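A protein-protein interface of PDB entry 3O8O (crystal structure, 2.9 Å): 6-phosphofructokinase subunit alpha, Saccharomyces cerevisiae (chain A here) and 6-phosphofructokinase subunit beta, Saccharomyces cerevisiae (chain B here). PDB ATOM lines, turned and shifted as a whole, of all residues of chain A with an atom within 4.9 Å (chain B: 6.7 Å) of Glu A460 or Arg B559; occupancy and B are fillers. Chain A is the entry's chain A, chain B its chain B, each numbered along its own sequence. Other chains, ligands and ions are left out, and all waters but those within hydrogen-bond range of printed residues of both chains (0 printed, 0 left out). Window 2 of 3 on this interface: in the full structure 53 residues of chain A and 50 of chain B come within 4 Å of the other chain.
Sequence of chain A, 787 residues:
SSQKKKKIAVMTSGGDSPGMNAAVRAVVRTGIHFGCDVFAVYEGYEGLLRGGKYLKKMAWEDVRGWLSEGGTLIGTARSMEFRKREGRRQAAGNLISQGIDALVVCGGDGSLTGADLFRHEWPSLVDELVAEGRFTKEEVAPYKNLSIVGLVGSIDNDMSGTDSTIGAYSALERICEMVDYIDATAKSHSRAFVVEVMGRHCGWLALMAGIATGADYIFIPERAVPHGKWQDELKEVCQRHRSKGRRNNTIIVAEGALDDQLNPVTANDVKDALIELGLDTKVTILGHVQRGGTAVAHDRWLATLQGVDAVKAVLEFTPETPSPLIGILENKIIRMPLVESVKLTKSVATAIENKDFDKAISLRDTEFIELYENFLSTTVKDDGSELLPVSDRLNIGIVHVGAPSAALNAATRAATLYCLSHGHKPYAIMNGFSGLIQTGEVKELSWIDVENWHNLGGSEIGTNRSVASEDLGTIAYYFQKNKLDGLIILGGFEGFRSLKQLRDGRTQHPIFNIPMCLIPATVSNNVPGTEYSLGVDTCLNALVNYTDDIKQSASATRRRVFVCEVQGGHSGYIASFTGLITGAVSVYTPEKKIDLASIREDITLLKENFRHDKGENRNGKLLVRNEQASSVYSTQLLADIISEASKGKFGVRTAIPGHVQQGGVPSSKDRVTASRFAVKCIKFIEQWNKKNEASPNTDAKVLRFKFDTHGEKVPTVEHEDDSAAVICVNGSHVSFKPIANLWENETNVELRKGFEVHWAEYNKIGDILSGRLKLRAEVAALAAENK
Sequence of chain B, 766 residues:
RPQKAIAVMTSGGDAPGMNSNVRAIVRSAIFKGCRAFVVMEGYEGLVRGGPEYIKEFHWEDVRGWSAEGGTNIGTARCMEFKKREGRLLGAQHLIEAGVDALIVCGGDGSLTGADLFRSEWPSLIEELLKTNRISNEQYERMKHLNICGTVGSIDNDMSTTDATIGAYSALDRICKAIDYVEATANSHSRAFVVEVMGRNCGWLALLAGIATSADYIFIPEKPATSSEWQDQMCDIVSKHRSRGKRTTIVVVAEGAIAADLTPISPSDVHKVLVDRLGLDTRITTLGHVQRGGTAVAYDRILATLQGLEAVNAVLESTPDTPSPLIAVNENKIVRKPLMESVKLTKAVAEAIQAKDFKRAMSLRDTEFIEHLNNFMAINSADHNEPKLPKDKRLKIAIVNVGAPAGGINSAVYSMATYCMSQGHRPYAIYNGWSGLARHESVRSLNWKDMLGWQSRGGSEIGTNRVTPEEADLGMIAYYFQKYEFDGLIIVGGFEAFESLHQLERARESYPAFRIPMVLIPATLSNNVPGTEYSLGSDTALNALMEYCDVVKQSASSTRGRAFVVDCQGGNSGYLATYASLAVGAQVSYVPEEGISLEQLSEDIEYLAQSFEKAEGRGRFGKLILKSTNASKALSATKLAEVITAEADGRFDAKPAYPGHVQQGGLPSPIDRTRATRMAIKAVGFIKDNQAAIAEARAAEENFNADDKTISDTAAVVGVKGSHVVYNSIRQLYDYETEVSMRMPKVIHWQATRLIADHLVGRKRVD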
ATOM      1  N   ASN A 409      -3.827  37.722  15.337  1.00  0.00           N
ATOM      2  CA  ASN A 409      -4.401  38.745  14.475  1.00  0.00           C
ATOM      3  C   ASN A 409      -4.058  40.141  14.980  1.00  0.00           C
ATOM      4  O   ASN A 409      -3.637  40.991  14.212  1.00  0.00           O
ATOM      5  CB  ASN A 409      -5.917  38.583  14.362  1.00  0.00           C
ATOM      6  CG  ASN A 409      -6.315  37.277  13.724  1.00  0.00           C
ATOM      7  OD1 ASN A 409      -5.687  36.847  12.768  1.00  0.00           O
ATOM      8  ND2 ASN A 409      -7.371  36.647  14.234  1.00  0.00           N
ATOM      9  N   MET A 430       0.387  32.827   3.957  1.00  0.00           N
ATOM     10  CA  MET A 430      -0.752  32.004   4.318  1.00  0.00           C
ATOM     11  C   MET A 430      -0.468  30.569   4.796  1.00  0.00           C
ATOM     12  O   MET A 430       0.422  29.884   4.295  1.00  0.00           O
ATOM     13  CB  MET A 430      -1.718  31.966   3.144  1.00  0.00           C
ATOM     14  CG  MET A 430      -2.017  33.335   2.561  1.00  0.00           C
ATOM     15  SD  MET A 430      -2.794  34.458   3.751  1.00  0.00           S
ATOM     16  CE  MET A 430      -4.431  33.757   3.956  1.00  0.00           C
ATOM     17  N   ASN A 431      -1.253  30.140   5.778  1.00  0.00           N
ATOM     18  CA  ASN A 431      -1.184  28.804   6.345  1.00  0.00           C
ATOM     19  C   ASN A 431       0.157  28.250   6.768  1.00  0.00           C
ATOM     20  O   ASN A 431       0.497  27.116   6.427  1.00  0.00           O
ATOM     21  CB  ASN A 431      -1.801  27.830   5.388  1.00  0.00           C
ATOM     22  CG  ASN A 431      -3.167  28.243   4.965  1.00  0.00           C
ATOM     23  OD1 ASN A 431      -4.094  28.297   5.782  1.00  0.00           O
ATOM     24  ND2 ASN A 431      -3.318  28.544   3.671  1.00  0.00           N
ATOM     25  N   TRP A 453      -8.969  43.329  13.528  1.00  0.00           N
ATOM     26  CA  TRP A 453      -8.232  42.135  13.891  1.00  0.00           C
ATOM     27  C   TRP A 453      -7.801  42.255  15.342  1.00  0.00           C
ATOM     28  O   TRP A 453      -7.548  41.251  15.998  1.00  0.00           O
ATOM     29  CB  TRP A 453      -7.005  41.959  13.003  1.00  0.00           C
ATOM     30  CG  TRP A 453      -7.319  41.276  11.724  1.00  0.00           C
ATOM     31  CD1 TRP A 453      -8.544  41.130  11.158  1.00  0.00           C
ATOM     32  CD2 TRP A 453      -6.382  40.712  10.802  1.00  0.00           C
ATOM     33  NE1 TRP A 453      -8.434  40.521   9.940  1.00  0.00           N
ATOM     34  CE2 TRP A 453      -7.116  40.253   9.693  1.00  0.00           C
ATOM     35  CE3 TRP A 453      -4.988  40.553  10.806  1.00  0.00           C
ATOM     36  CZ2 TRP A 453      -6.508  39.648   8.592  1.00  0.00           C
ATOM     37  CZ3 TRP A 453      -4.381  39.951   9.712  1.00  0.00           C
ATOM     38  CH2 TRP A 453      -5.142  39.507   8.620  1.00  0.00           C
ATOM     39  N   LEU A 456      -9.826  39.972  17.400  1.00  0.00           N
ATOM     40  CA  LEU A 456     -10.189  38.736  16.740  1.00  0.00           C
ATOM     41  C   LEU A 456      -9.272  37.578  17.129  1.00  0.00           C
ATOM     42  O   LEU A 456      -8.073  37.600  16.835  1.00  0.00           O
ATOM     43  CB  LEU A 456     -10.093  38.958  15.259  1.00  0.00           C
ATOM     44  CG  LEU A 456     -11.279  38.523  14.419  1.00  0.00           C
ATOM     45  CD1 LEU A 456     -10.790  38.513  12.952  1.00  0.00           C
ATOM     46  CD2 LEU A 456     -11.794  37.146  14.884  1.00  0.00           C
ATOM     47  N   GLY A 458      -7.957  33.477  17.242  1.00  0.00           N
ATOM     48  CA  GLY A 458      -7.610  32.555  16.174  1.00  0.00           C
ATOM     49  C   GLY A 458      -6.612  33.152  15.204  1.00  0.00           C
ATOM     50  O   GLY A 458      -5.917  34.101  15.561  1.00  0.00           O
ATOM     51  N   SER A 459      -6.552  32.606  13.993  1.00  0.00           N
ATOM     52  CA  SER A 459      -5.639  33.101  12.975  1.00  0.00           C
ATOM     53  C   SER A 459      -6.290  33.288  11.609  1.00  0.00           C
ATOM     54  O   SER A 459      -6.520  32.320  10.886  1.00  0.00           O
ATOM     55  CB  SER A 459      -4.438  32.160  12.813  1.00  0.00           C
ATOM     56  OG  SER A 459      -3.656  32.547  11.695  1.00  0.00           O
ATOM     57  N   GLU A 460      -6.559  34.533  11.242  1.00  0.00           N
ATOM     58  CA  GLU A 460      -7.172  34.823   9.953  1.00  0.00           C
ATOM     59  C   GLU A 460      -6.361  34.347   8.731  1.00  0.00           C
ATOM     60  O   GLU A 460      -6.940  34.020   7.691  1.00  0.00           O
ATOM     61  CB  GLU A 460      -7.458  36.328   9.833  1.00  0.00           C
ATOM     62  CG  GLU A 460      -8.610  36.834  10.696  1.00  0.00           C
ATOM     63  CD  GLU A 460      -9.957  36.216  10.333  1.00  0.00           C
ATOM     64  OE1 GLU A 460     -10.352  36.297   9.156  1.00  0.00           O
ATOM     65  OE2 GLU A 460     -10.633  35.663  11.226  1.00  0.00           O
ATOM     66  N   ILE A 461      -5.040  34.307   8.835  1.00  0.00           N
ATOM     67  CA  ILE A 461      -4.245  33.872   7.697  1.00  0.00           C
ATOM     68  C   ILE A 461      -3.937  32.379   7.760  1.00  0.00           C
ATOM     69  O   ILE A 461      -3.439  31.797   6.802  1.00  0.00           O
ATOM     70  CB  ILE A 461      -2.917  34.648   7.606  1.00  0.00           C
ATOM     71  CG1 ILE A 461      -2.091  34.427   8.889  1.00  0.00           C
ATOM     72  CG2 ILE A 461      -3.202  36.139   7.355  1.00  0.00           C
ATOM     73  CD1 ILE A 461      -0.767  35.220   8.949  1.00  0.00           C
ATOM     74  N   GLY A 462      -4.243  31.754   8.887  1.00  0.00           N
ATOM     75  CA  GLY A 462      -3.981  30.338   9.028  1.00  0.00           C
ATOM     76  C   GLY A 462      -2.712  30.060   9.815  1.00  0.00           C
ATOM     77  O   GLY A 462      -1.674  30.705   9.627  1.00  0.00           O
ATOM     78  N   GLN B 553     -13.789  28.685  16.182  1.00  0.00           N
ATOM     79  CA  GLN B 553     -12.848  29.712  15.763  1.00  0.00           C
ATOM     80  C   GLN B 553     -11.481  29.058  15.701  1.00  0.00           C
ATOM     81  O   GLN B 553     -10.667  29.338  14.840  1.00  0.00           O
ATOM     82  CB  GLN B 553     -12.817  30.833  16.778  1.00  0.00           C
ATOM     83  CG  GLN B 553     -11.980  31.994  16.369  1.00  0.00           C
ATOM     84  CD  GLN B 553     -11.775  32.914  17.511  1.00  0.00           C
ATOM     85  OE1 GLN B 553     -12.212  34.066  17.485  1.00  0.00           O
ATOM     86  NE2 GLN B 553     -11.123  32.417  18.548  1.00  0.00           N
ATOM     87  N   SER B 554     -11.231  28.174  16.646  1.00  0.00           N
ATOM     88  CA  SER B 554      -9.966  27.467  16.693  1.00  0.00           C
ATOM     89  C   SER B 554      -9.832  26.684  15.406  1.00  0.00           C
ATOM     90  O   SER B 554      -8.890  26.869  14.631  1.00  0.00           O
ATOM     91  CB  SER B 554      -9.970  26.508  17.884  1.00  0.00           C
ATOM     92  OG  SER B 554      -8.803  25.721  17.944  1.00  0.00           O
ATOM     93  N   ALA B 555     -10.809  25.820  15.180  1.00  0.00           N
ATOM     94  CA  ALA B 555     -10.829  24.978  14.003  1.00  0.00           C
ATOM     95  C   ALA B 555     -10.676  25.735  12.721  1.00  0.00           C
ATOM     96  O   ALA B 555     -10.124  25.215  11.767  1.00  0.00           O
ATOM     97  CB  ALA B 555     -12.090  24.209  13.960  1.00  0.00           C
ATOM     98  N   SER B 556     -11.188  26.954  12.674  1.00  0.00           N
ATOM     99  CA  SER B 556     -11.103  27.730  11.454  1.00  0.00           C
ATOM    100  C   SER B 556      -9.719  28.263  11.274  1.00  0.00           C
ATOM    101  O   SER B 556      -9.297  28.546  10.158  1.00  0.00           O
ATOM    102  CB  SER B 556     -12.115  28.881  11.463  1.00  0.00           C
ATOM    103  OG  SER B 556     -13.411  28.424  11.120  1.00  0.00           O
ATOM    104  N   SER B 557      -9.006  28.386  12.381  1.00  0.00           N
ATOM    105  CA  SER B 557      -7.665  28.917  12.350  1.00  0.00           C
ATOM    106  C   SER B 557      -6.659  27.955  11.739  1.00  0.00           C
ATOM    107  O   SER B 557      -5.727  28.369  11.035  1.00  0.00           O
ATOM    108  CB  SER B 557      -7.230  29.281  13.765  1.00  0.00           C
ATOM    109  OG  SER B 557      -8.021  30.335  14.248  1.00  0.00           O
ATOM    110  N   THR B 558      -6.850  26.674  12.019  1.00  0.00           N
ATOM    111  CA  THR B 558      -5.944  25.645  11.531  1.00  0.00           C
ATOM    112  C   THR B 558      -6.255  25.273  10.094  1.00  0.00           C
ATOM    113  O   THR B 558      -5.365  24.894   9.352  1.00  0.00           O
ATOM    114  CB  THR B 558      -6.040  24.375  12.413  1.00  0.00           C
ATOM    115  OG1 THR B 558      -5.716  24.708  13.765  1.00  0.00           O
ATOM    116  CG2 THR B 558      -5.087  23.317  11.934  1.00  0.00           C
ATOM    117  N   ARG B 559      -7.524  25.395   9.726  1.00  0.00           N
ATOM    118  CA  ARG B 559      -8.011  25.045   8.398  1.00  0.00           C
ATOM    119  C   ARG B 559      -8.030  23.526   8.264  1.00  0.00           C
ATOM    120  O   ARG B 559      -7.097  22.838   8.691  1.00  0.00           O
ATOM    121  CB  ARG B 559      -7.126  25.627   7.293  1.00  0.00           C
ATOM    122  CG  ARG B 559      -6.604  26.986   7.566  1.00  0.00           C
ATOM    123  CD  ARG B 559      -7.401  28.078   6.939  1.00  0.00           C
ATOM    124  NE  ARG B 559      -7.269  29.259   7.790  1.00  0.00           N
ATOM    125  CZ  ARG B 559      -7.100  30.502   7.363  1.00  0.00           C
ATOM    126  NH1 ARG B 559      -7.049  30.764   6.066  1.00  0.00           N
ATOM    127  NH2 ARG B 559      -6.939  31.474   8.249  1.00  0.00           N
ATOM    128  N   GLY B 560      -9.089  23.001   7.663  1.00  0.00           N
ATOM    129  CA  GLY B 560      -9.168  21.567   7.494  1.00  0.00           C
ATOM    130  C   GLY B 560      -9.197  20.847   8.827  1.00  0.00           C
ATOM    131  O   GLY B 560      -8.424  19.920   9.085  1.00  0.00           O
ATOM    132  N   ARG B 561     -10.092  21.284   9.698  1.00  0.00           N
ATOM    133  CA  ARG B 561     -10.214  20.642  10.982  1.00  0.00           C
ATOM    134  C   ARG B 561     -11.612  20.746  11.527  1.00  0.00           C
ATOM    135  O   ARG B 561     -12.271  21.765  11.377  1.00  0.00           O
ATOM    136  CB  ARG B 561      -9.237  21.245  11.982  1.00  0.00           C
ATOM    137  CG  ARG B 561      -9.524  20.795  13.386  1.00  0.00           C
ATOM    138  CD  ARG B 561      -8.370  21.049  14.276  1.00  0.00           C
ATOM    139  NE  ARG B 561      -7.251  20.152  14.011  1.00  0.00           N
ATOM    140  CZ  ARG B 561      -6.143  20.136  14.747  1.00  0.00           C
ATOM    141  NH1 ARG B 561      -6.024  20.963  15.772  1.00  0.00           N
ATOM    142  NH2 ARG B 561      -5.162  19.297  14.470  1.00  0.00           N
ATOM    143  N   PHE B 611     -14.212  20.552   3.202  1.00  0.00           N
ATOM    144  CA  PHE B 611     -12.895  21.155   3.260  1.00  0.00           C
ATOM    145  C   PHE B 611     -12.215  21.283   1.914  1.00  0.00           C
ATOM    146  O   PHE B 611     -11.429  22.196   1.707  1.00  0.00           O
ATOM    147  CB  PHE B 611     -11.997  20.368   4.193  1.00  0.00           C
ATOM    148  CG  PHE B 611     -12.384  20.474   5.618  1.00  0.00           C
ATOM    149  CD1 PHE B 611     -12.886  19.370   6.314  1.00  0.00           C
ATOM    150  CD2 PHE B 611     -12.271  21.685   6.273  1.00  0.00           C
ATOM    151  CE1 PHE B 611     -13.269  19.485   7.664  1.00  0.00           C
ATOM    152  CE2 PHE B 611     -12.648  21.810   7.602  1.00  0.00           C
ATOM    153  CZ  PHE B 611     -13.148  20.712   8.304  1.00  0.00           C
ATOM    154  N   GLU B 615     -11.068  24.877   0.204  1.00  0.00           N
ATOM    155  CA  GLU B 615      -9.670  25.190  -0.083  1.00  0.00           C
ATOM    156  C   GLU B 615      -9.023  25.577   1.244  1.00  0.00           C
ATOM    157  O   GLU B 615      -9.324  24.973   2.289  1.00  0.00           O
ATOM    158  CB  GLU B 615      -9.563  26.344  -1.073  1.00  0.00           C
ATOM    159  CG  GLU B 615     -10.662  26.321  -2.128  1.00  0.00           C
ATOM    160  CD  GLU B 615     -10.126  26.227  -3.547  1.00  0.00           C
ATOM    161  OE1 GLU B 615     -10.945  26.399  -4.491  1.00  0.00           O
ATOM    162  OE2 GLU B 615      -8.901  25.979  -3.711  1.00  0.00           O
ATOM    163  N   GLY B 616      -8.152  26.585   1.228  1.00  0.00           N
ATOM    164  CA  GLY B 616      -7.507  26.976   2.474  1.00  0.00           C
ATOM    165  C   GLY B 616      -8.166  28.143   3.183  1.00  0.00           C
ATOM    166  O   GLY B 616      -7.634  28.640   4.178  1.00  0.00           O
ATOM    167  N   ARG B 617      -9.326  28.564   2.675  1.00  0.00           N
ATOM    168  CA  ARG B 617     -10.058  29.699   3.220  1.00  0.00           C
ATOM    169  C   ARG B 617     -10.136  29.817   4.738  1.00  0.00           C
ATOM    170  O   ARG B 617     -10.090  28.822   5.469  1.00  0.00           O
ATOM    171  CB  ARG B 617     -11.463  29.771   2.621  1.00  0.00           C
ATOM    172  CG  ARG B 617     -11.610  30.855   1.574  1.00  0.00           C
ATOM    173  CD  ARG B 617     -11.356  30.297   0.219  1.00  0.00           C
ATOM    174  NE  ARG B 617     -12.403  29.352  -0.139  1.00  0.00           N
ATOM    175  CZ  ARG B 617     -13.653  29.703  -0.396  1.00  0.00           C
ATOM    176  NH1 ARG B 617     -13.998  30.982  -0.321  1.00  0.00           N
ATOM    177  NH2 ARG B 617     -14.536  28.783  -0.768  1.00  0.00           N
ATOM    178  N   GLY B 618     -10.299  31.065   5.172  1.00  0.00           N
ATOM    179  CA  GLY B 618     -10.322  31.433   6.576  1.00  0.00           C
ATOM    180  C   GLY B 618     -11.410  31.170   7.602  1.00  0.00           C
ATOM    181  O   GLY B 618     -11.107  31.266   8.796  1.00  0.00           O
ATOM    182  N   ARG B 619     -12.649  30.876   7.225  1.00  0.00           N
ATOM    183  CA  ARG B 619     -13.624  30.632   8.295  1.00  0.00           C
ATOM    184  C   ARG B 619     -14.428  29.386   8.037  1.00  0.00           C
ATOM    185  O   ARG B 619     -15.650  29.397   8.172  1.00  0.00           O
ATOM    186  CB  ARG B 619     -14.559  31.846   8.498  1.00  0.00           C
ATOM    187  N   PHE B 620     -13.720  28.304   7.695  1.00  0.00           N
ATOM    188  CA  PHE B 620     -14.343  27.025   7.382  1.00  0.00           C
ATOM    189  C   PHE B 620     -14.169  25.914   8.403  1.00  0.00           C
ATOM    190  O   PHE B 620     -14.218  24.755   8.039  1.00  0.00           O
ATOM    191  CB  PHE B 620     -13.854  26.525   6.014  1.00  0.00           C
ATOM    192  CG  PHE B 620     -14.549  27.171   4.842  1.00  0.00           C
ATOM    193  CD1 PHE B 620     -13.913  28.134   4.074  1.00  0.00           C
ATOM    194  CD2 PHE B 620     -15.858  26.835   4.526  1.00  0.00           C
ATOM    195  CE1 PHE B 620     -14.568  28.763   3.002  1.00  0.00           C
ATOM    196  CE2 PHE B 620     -16.517  27.463   3.457  1.00  0.00           C
ATOM    197  CZ  PHE B 620     -15.864  28.430   2.699  1.00  0.00           C
ATOM    198  N   GLY B 621     -13.975  26.251   9.673  1.00  0.00           N
ATOM    199  CA  GLY B 621     -13.831  25.217  10.683  1.00  0.00           C
ATOM    200  C   GLY B 621     -15.179  24.535  10.847  1.00  0.00           C
ATOM    201  O   GLY B 621     -16.211  25.184  10.662  1.00  0.00           O
ATOM    202  N   PHE B 651      -8.380  15.882   6.095  1.00  0.00           N
ATOM    203  CA  PHE B 651      -8.691  16.808   7.184  1.00  0.00           C
ATOM    204  C   PHE B 651      -8.650  15.980   8.457  1.00  0.00           C
ATOM    205  O   PHE B 651      -8.675  14.758   8.386  1.00  0.00           O
ATOM    206  CB  PHE B 651     -10.087  17.397   7.005  1.00  0.00           C
ATOM    207  CG  PHE B 651     -11.177  16.398   7.177  1.00  0.00           C
ATOM    208  CD1 PHE B 651     -11.882  16.323   8.376  1.00  0.00           C
ATOM    209  CD2 PHE B 651     -11.528  15.526   6.136  1.00  0.00           C
ATOM    210  CE1 PHE B 651     -12.941  15.392   8.546  1.00  0.00           C
ATOM    211  CE2 PHE B 651     -12.586  14.587   6.292  1.00  0.00           C
ATOM    212  CZ  PHE B 651     -13.288  14.528   7.497  1.00  0.00           C
ATOM    213  N   ASP B 652      -8.565  16.612   9.622  1.00  0.00           N
ATOM    214  CA  ASP B 652      -8.559  15.819  10.841  1.00  0.00           C
ATOM    215  C   ASP B 652      -9.624  16.306  11.818  1.00  0.00           C
ATOM    216  O   ASP B 652     -10.384  17.251  11.522  1.00  0.00           O
ATOM    217  CB  ASP B 652      -7.202  15.859  11.517  1.00  0.00           C
ATOM    218  CG  ASP B 652      -6.872  17.228  12.036  1.00  0.00           C
ATOM    219  OD1 ASP B 652      -5.905  17.392  12.825  1.00  0.00           O
ATOM    220  OD2 ASP B 652      -7.597  18.158  11.641  1.00  0.00           O
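NH2 of Arg B559 sits close to N of Gly A462 (2.8 Å). The backbone carbonyl oxygen of Glu A460 is in hydrogen-bond range of the guanidinium group of Arg B559, at 2.6 Å. O of Ser A459 sits at hydrogen-bond distance from NH2 of Arg B559, at 2.8 Å. The guanidinium group (NH2) of Arg B559 sits close to the backbone NH (N) of Ile A461 (3.5 Å). The backbone NH (N) of Ser A459 sits at hydrogen-bond distance from the side-chain hydroxyl (OG) of Ser B557 (2.7 Å).
OG of Ser A459 is in hydrogen-bond range of N of Gly A462 (3.0 Å). The side-chain hydroxyl (OG) of Ser B557 lies within hydrogen-bond range of the backbone carbonyl oxygen (O) of Gln B553, 2.9 Å away. OD1 of Asn A409 is in hydrogen-bond range of N of Glu A460. The backbone NH (N) of Asn A431 lies within hydrogen-bond range of the backbone carbonyl oxygen (O) of Ile A461 (2.9 Å). The guanidinium group (NH1) of Arg B559 lies close to the backbone carbonyl oxygen (O) of Gly B616, at 2.9 Å. The side-chain amide nitrogen of Asn A409 is in hydrogen-bond range of the backbone carbonyl oxygen of Gly A458, 3.2 Å away.
OD1 of Asn A431 touches CG of Arg B559, 3.3 Å away. Gly B616 touches Asn A431. N of Gly A458 touches NE2 of Gln B553, at 3.6 Å. Ser B557 touches Gly A458 (OG to CA, 3.0 Å). Gly A462 touches Ser B557.
Met A430 touches none of the printed residues of chain B. Of the printed residues of chain B, Asn A431 touches Arg B559 (3.3 Å) and Gly B616 (3.9 Å). Of the printed residues of chain B, Gly A458 touches Gln B553 (3.6 Å) and Ser B557 (3.0 Å). Of chain B, only Arg B559 comes within 4 Å of Glu A460. Arg B559 touches just these residues of chain A: Asn A431 (3.3 Å), Ser A459 (2.8 Å), Glu A460 (2.6 Å), Ile A461 (3.2 Å) and Gly A462 (2.8 Å). Phe B611 touches none of the printed residues of chain A. Of the printed residues of chain A, Gly B616 touches Asn A431 (3.9 Å). The nearest residue of chain B that does not touch Glu A460 is Gly B618 (4.4 Å).
Of the 19 printed residues of chain B, 4 touch a printed residue of chain A. Of the 10 printed residues of chain A, 6 touch a printed residue of chain B. Among the printed residues, 10 pairs touch across the chains.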
